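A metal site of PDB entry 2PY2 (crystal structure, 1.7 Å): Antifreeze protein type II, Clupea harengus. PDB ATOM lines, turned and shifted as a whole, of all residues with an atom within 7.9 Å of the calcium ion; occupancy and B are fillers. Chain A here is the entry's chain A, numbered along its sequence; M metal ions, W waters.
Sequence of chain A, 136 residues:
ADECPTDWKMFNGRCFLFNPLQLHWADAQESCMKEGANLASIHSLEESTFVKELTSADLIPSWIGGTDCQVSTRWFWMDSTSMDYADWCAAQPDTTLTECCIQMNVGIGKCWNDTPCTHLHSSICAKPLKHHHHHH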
ATOM      1  N   TRP A  75     -21.570  19.124 -38.407  1.00  0.00           N
ATOM      2  CA  TRP A  75     -20.858  20.335 -38.044  1.00  0.00           C
ATOM      3  C   TRP A  75     -20.923  21.487 -39.039  1.00  0.00           C
ATOM      4  O   TRP A  75     -20.761  21.295 -40.248  1.00  0.00           O
ATOM      5  CB  TRP A  75     -19.395  19.997 -37.772  1.00  0.00           C
ATOM      6  CG  TRP A  75     -19.244  19.006 -36.680  1.00  0.00           C
ATOM      7  CD1 TRP A  75     -19.251  17.640 -36.804  1.00  0.00           C
ATOM      8  CD2 TRP A  75     -19.158  19.279 -35.283  1.00  0.00           C
ATOM      9  NE1 TRP A  75     -19.190  17.050 -35.572  1.00  0.00           N
ATOM     10  CE2 TRP A  75     -19.132  18.028 -34.613  1.00  0.00           C
ATOM     11  CE3 TRP A  75     -19.107  20.453 -34.522  1.00  0.00           C
ATOM     12  CZ2 TRP A  75     -19.060  17.931 -33.222  1.00  0.00           C
ATOM     13  CZ3 TRP A  75     -19.042  20.360 -33.137  1.00  0.00           C
ATOM     14  CH2 TRP A  75     -19.022  19.097 -32.502  1.00  0.00           C
ATOM     15  N   TRP A  88      -9.396  17.610 -33.390  1.00  0.00           N
ATOM     16  CA  TRP A  88      -9.999  17.011 -32.205  1.00  0.00           C
ATOM     17  C   TRP A  88      -9.029  16.343 -31.222  1.00  0.00           C
ATOM     18  O   TRP A  88      -8.066  15.687 -31.624  1.00  0.00           O
ATOM     19  CB  TRP A  88     -11.028  15.960 -32.620  1.00  0.00           C
ATOM     20  CG  TRP A  88     -12.159  16.481 -33.440  1.00  0.00           C
ATOM     21  CD1 TRP A  88     -12.476  16.144 -34.725  1.00  0.00           C
ATOM     22  CD2 TRP A  88     -13.152  17.433 -33.020  1.00  0.00           C
ATOM     23  NE1 TRP A  88     -13.616  16.816 -35.126  1.00  0.00           N
ATOM     24  CE2 TRP A  88     -14.048  17.604 -34.099  1.00  0.00           C
ATOM     25  CE3 TRP A  88     -13.374  18.140 -31.825  1.00  0.00           C
ATOM     26  CZ2 TRP A  88     -15.143  18.465 -34.023  1.00  0.00           C
ATOM     27  CZ3 TRP A  88     -14.468  18.992 -31.755  1.00  0.00           C
ATOM     28  CH2 TRP A  88     -15.335  19.150 -32.845  1.00  0.00           C
ATOM     29  N   ALA A  90      -8.137  13.599 -28.239  1.00  0.00           N
ATOM     30  CA  ALA A  90      -8.439  12.166 -28.204  1.00  0.00           C
ATOM     31  C   ALA A  90      -9.848  11.974 -27.665  1.00  0.00           C
ATOM     32  O   ALA A  90     -10.233  12.615 -26.686  1.00  0.00           O
ATOM     33  CB  ALA A  90      -7.427  11.442 -27.308  1.00  0.00           C
ATOM     34  N   ALA A  91     -10.618  11.103 -28.329  1.00  0.00           N
ATOM     35  CA  ALA A  91     -11.988  10.786 -27.936  1.00  0.00           C
ATOM     36  C   ALA A  91     -13.007  11.833 -28.375  1.00  0.00           C
ATOM     37  O   ALA A  91     -14.217  11.603 -28.286  1.00  0.00           O
ATOM     38  CB  ALA A  91     -12.078  10.568 -26.433  1.00  0.00           C
ATOM     39  N   GLN A  92     -12.537  12.976 -28.859  1.00  0.00           N
ATOM     40  CA  GLN A  92     -13.410  14.055 -29.308  1.00  0.00           C
ATOM     41  C   GLN A  92     -13.706  13.939 -30.791  1.00  0.00           C
ATOM     42  O   GLN A  92     -12.893  13.418 -31.545  1.00  0.00           O
ATOM     43  CB  GLN A  92     -12.743  15.399 -29.029  1.00  0.00           C
ATOM     44  CG  GLN A  92     -12.425  15.590 -27.562  1.00  0.00           C
ATOM     45  CD  GLN A  92     -13.678  15.639 -26.740  1.00  0.00           C
ATOM     46  OE1 GLN A  92     -14.516  16.508 -26.951  1.00  0.00           O
ATOM     47  NE2 GLN A  92     -13.835  14.705 -25.812  1.00  0.00           N
ATOM     48  N   PRO A  93     -14.887  14.413 -31.231  1.00  0.00           N
ATOM     49  CA  PRO A  93     -15.915  15.044 -30.396  1.00  0.00           C
ATOM     50  C   PRO A  93     -16.906  14.024 -29.817  1.00  0.00           C
ATOM     51  O   PRO A  93     -17.043  12.917 -30.341  1.00  0.00           O
ATOM     52  CB  PRO A  93     -16.598  16.012 -31.366  1.00  0.00           C
ATOM     53  CG  PRO A  93     -16.609  15.214 -32.634  1.00  0.00           C
ATOM     54  CD  PRO A  93     -15.199  14.595 -32.662  1.00  0.00           C
ATOM     55  N   ASP A  94     -17.604  14.381 -28.742  1.00  0.00           N
ATOM     56  CA  ASP A  94     -18.582  13.464 -28.167  1.00  0.00           C
ATOM     57  C   ASP A  94     -19.870  13.441 -29.009  1.00  0.00           C
ATOM     58  O   ASP A  94     -20.564  12.426 -29.063  1.00  0.00           O
ATOM     59  CB  ASP A  94     -18.881  13.857 -26.724  1.00  0.00           C
ATOM     60  CG  ASP A  94     -17.706  13.588 -25.801  1.00  0.00           C
ATOM     61  OD1 ASP A  94     -17.398  12.407 -25.549  1.00  0.00           O
ATOM     62  OD2 ASP A  94     -17.075  14.545 -25.339  1.00  0.00           O
ATOM     63  N   THR A  95     -20.141  14.566 -29.672  1.00  0.00           N
ATOM     64  CA  THR A  95     -21.318  14.765 -30.533  1.00  0.00           C
ATOM     65  C   THR A  95     -22.638  14.863 -29.786  1.00  0.00           C
ATOM     66  O   THR A  95     -23.713  14.898 -30.412  1.00  0.00           O
ATOM     67  CB  THR A  95     -21.465  13.684 -31.651  1.00  0.00           C
ATOM     68  OG1 THR A  95     -21.958  12.457 -31.089  1.00  0.00           O
ATOM     69  CG2 THR A  95     -20.112  13.420 -32.338  1.00  0.00           C
ATOM     70  N   THR A  96     -22.571  14.935 -28.456  1.00  0.00           N
ATOM     71  CA  THR A  96     -23.774  15.061 -27.632  1.00  0.00           C
ATOM     72  C   THR A  96     -24.292  16.482 -27.812  1.00  0.00           C
ATOM     73  O   THR A  96     -23.515  17.434 -27.765  1.00  0.00           O
ATOM     74  CB  THR A  96     -23.476  14.869 -26.137  1.00  0.00           C
ATOM     75  OG1 THR A  96     -22.596  13.746 -25.966  1.00  0.00           O
ATOM     76  CG2 THR A  96     -24.755  14.625 -25.361  1.00  0.00           C
ATOM     77  N   GLU A  99     -23.191  19.383 -25.457  1.00  0.00           N
ATOM     78  CA  GLU A  99     -21.837  19.951 -25.499  1.00  0.00           C
ATOM     79  C   GLU A  99     -21.519  20.059 -26.978  1.00  0.00           C
ATOM     80  O   GLU A  99     -20.638  19.367 -27.492  1.00  0.00           O
ATOM     81  CB  GLU A  99     -20.870  18.994 -24.798  1.00  0.00           C
ATOM     82  CG  GLU A  99     -20.870  17.595 -25.384  1.00  0.00           C
ATOM     83  CD  GLU A  99     -20.119  16.581 -24.530  1.00  0.00           C
ATOM     84  OE1 GLU A  99     -19.000  16.906 -24.082  1.00  0.00           O
ATOM     85  OE2 GLU A  99     -20.653  15.476 -24.324  1.00  0.00           O
ATOM     86  N   CYS A 100     -22.214  20.972 -27.655  1.00  0.00           N
ATOM     87  CA  CYS A 100     -22.095  21.081 -29.107  1.00  0.00           C
ATOM     88  C   CYS A 100     -21.311  22.225 -29.743  1.00  0.00           C
ATOM     89  O   CYS A 100     -21.308  22.346 -30.971  1.00  0.00           O
ATOM     90  CB  CYS A 100     -23.519  21.047 -29.679  1.00  0.00           C
ATOM     91  SG  CYS A 100     -24.599  22.373 -29.035  1.00  0.00           S
ATOM     92  N   CYS A 101     -20.630  23.042 -28.932  1.00  0.00           N
ATOM     93  CA  CYS A 101     -19.847  24.176 -29.435  1.00  0.00           C
ATOM     94  C   CYS A 101     -18.359  23.823 -29.395  1.00  0.00           C
ATOM     95  O   CYS A 101     -17.897  23.227 -28.432  1.00  0.00           O
ATOM     96  CB  CYS A 101     -20.128  25.412 -28.578  1.00  0.00           C
ATOM     97  SG  CYS A 101     -21.757  26.161 -28.936  1.00  0.00           S
ATOM     98  N   TRP A 112      -9.039  20.478 -30.043  1.00  0.00           N
ATOM     99  CA  TRP A 112     -10.464  20.830 -30.008  1.00  0.00           C
ATOM    100  C   TRP A 112     -11.291  19.859 -29.172  1.00  0.00           C
ATOM    101  O   TRP A 112     -11.049  18.653 -29.146  1.00  0.00           O
ATOM    102  CB  TRP A 112     -11.069  20.862 -31.404  1.00  0.00           C
ATOM    103  CG  TRP A 112     -10.490  21.845 -32.369  1.00  0.00           C
ATOM    104  CD1 TRP A 112      -9.413  22.666 -32.177  1.00  0.00           C
ATOM    105  CD2 TRP A 112     -10.912  22.053 -33.714  1.00  0.00           C
ATOM    106  NE1 TRP A 112      -9.152  23.374 -33.328  1.00  0.00           N
ATOM    107  CE2 TRP A 112     -10.065  23.009 -34.290  1.00  0.00           C
ATOM    108  CE3 TRP A 112     -11.948  21.516 -34.489  1.00  0.00           C
ATOM    109  CZ2 TRP A 112     -10.198  23.440 -35.617  1.00  0.00           C
ATOM    110  CZ3 TRP A 112     -12.088  21.942 -35.810  1.00  0.00           C
ATOM    111  CH2 TRP A 112     -11.213  22.892 -36.357  1.00  0.00           C
ATOM    112  N   ASN A 113     -12.311  20.412 -28.535  1.00  0.00           N
ATOM    113  CA  ASN A 113     -13.189  19.637 -27.685  1.00  0.00           C
ATOM    114  C   ASN A 113     -14.589  20.248 -27.830  1.00  0.00           C
ATOM    115  O   ASN A 113     -14.719  21.470 -27.762  1.00  0.00           O
ATOM    116  CB  ASN A 113     -12.695  19.768 -26.252  1.00  0.00           C
ATOM    117  CG  ASN A 113     -13.401  18.862 -25.304  1.00  0.00           C
ATOM    118  OD1 ASN A 113     -14.628  18.860 -25.222  1.00  0.00           O
ATOM    119  ND2 ASN A 113     -12.639  18.080 -24.544  1.00  0.00           N
ATOM    120  N   ASP A 114     -15.631  19.443 -28.073  1.00  0.00           N
ATOM    121  CA  ASP A 114     -16.955  20.063 -28.136  1.00  0.00           C
ATOM    122  C   ASP A 114     -17.387  20.238 -26.681  1.00  0.00           C
ATOM    123  O   ASP A 114     -17.248  19.345 -25.859  1.00  0.00           O
ATOM    124  CB  ASP A 114     -17.969  19.259 -29.019  1.00  0.00           C
ATOM    125  CG  ASP A 114     -18.042  17.766 -28.707  1.00  0.00           C
ATOM    126  OD1 ASP A 114     -17.146  17.197 -28.069  1.00  0.00           O
ATOM    127  OD2 ASP A 114     -19.018  17.137 -29.148  1.00  0.00           O
ATOM    128  N   THR A 115     -17.865  21.431 -26.328  1.00  0.00           N
ATOM    129  CA  THR A 115     -18.210  21.683 -24.935  1.00  0.00           C
ATOM    130  C   THR A 115     -19.511  22.444 -24.781  1.00  0.00           C
ATOM    131  O   THR A 115     -19.995  23.042 -25.733  1.00  0.00           O
ATOM    132  CB  THR A 115     -17.011  22.418 -24.207  1.00  0.00           C
ATOM    133  OG1 THR A 115     -17.345  23.770 -23.884  1.00  0.00           O
ATOM    134  CG2 THR A 115     -15.774  22.401 -25.074  1.00  0.00           C
ATOM    135  N   PRO A 116     -20.121  22.388 -23.592  1.00  0.00           N
ATOM    136  CA  PRO A 116     -21.378  23.110 -23.364  1.00  0.00           C
ATOM    137  C   PRO A 116     -21.224  24.575 -23.763  1.00  0.00           C
ATOM    138  O   PRO A 116     -20.332  25.274 -23.292  1.00  0.00           O
ATOM    139  CB  PRO A 116     -21.612  22.922 -21.868  1.00  0.00           C
ATOM    140  CG  PRO A 116     -21.020  21.559 -21.622  1.00  0.00           C
ATOM    141  CD  PRO A 116     -19.725  21.607 -22.402  1.00  0.00           C
HETATM  142 CA    CA M   1     -16.671  16.978 -25.672  1.00  0.00          CA
HETATM  143  O   HOH W   1     -15.491  17.207 -23.314  1.00  0.00           O
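OD2 of Asp 114 is in hydrogen-bond range of N of Thr 95 (2.9 Å). The side-chain carboxylate of Glu 99 is in hydrogen-bond range of the side-chain hydroxyl of Thr 96, 3.1 Å away.
The nearest printed residue that does not touch the calcium ion is Thr 115 (4.7 Å).
The calcium ion is bound by O of Asp 114 (2.4 Å), OD1 of Asp 114 (2.5 Å), OD2 of Asp 94 (2.5 Å), OE1 of Gln 92 (2.5 Å), water W1 (2.6 Å), OD1 of Asn 113 (2.8 Å) and OE1 of Glu 99 (2.8 Å).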
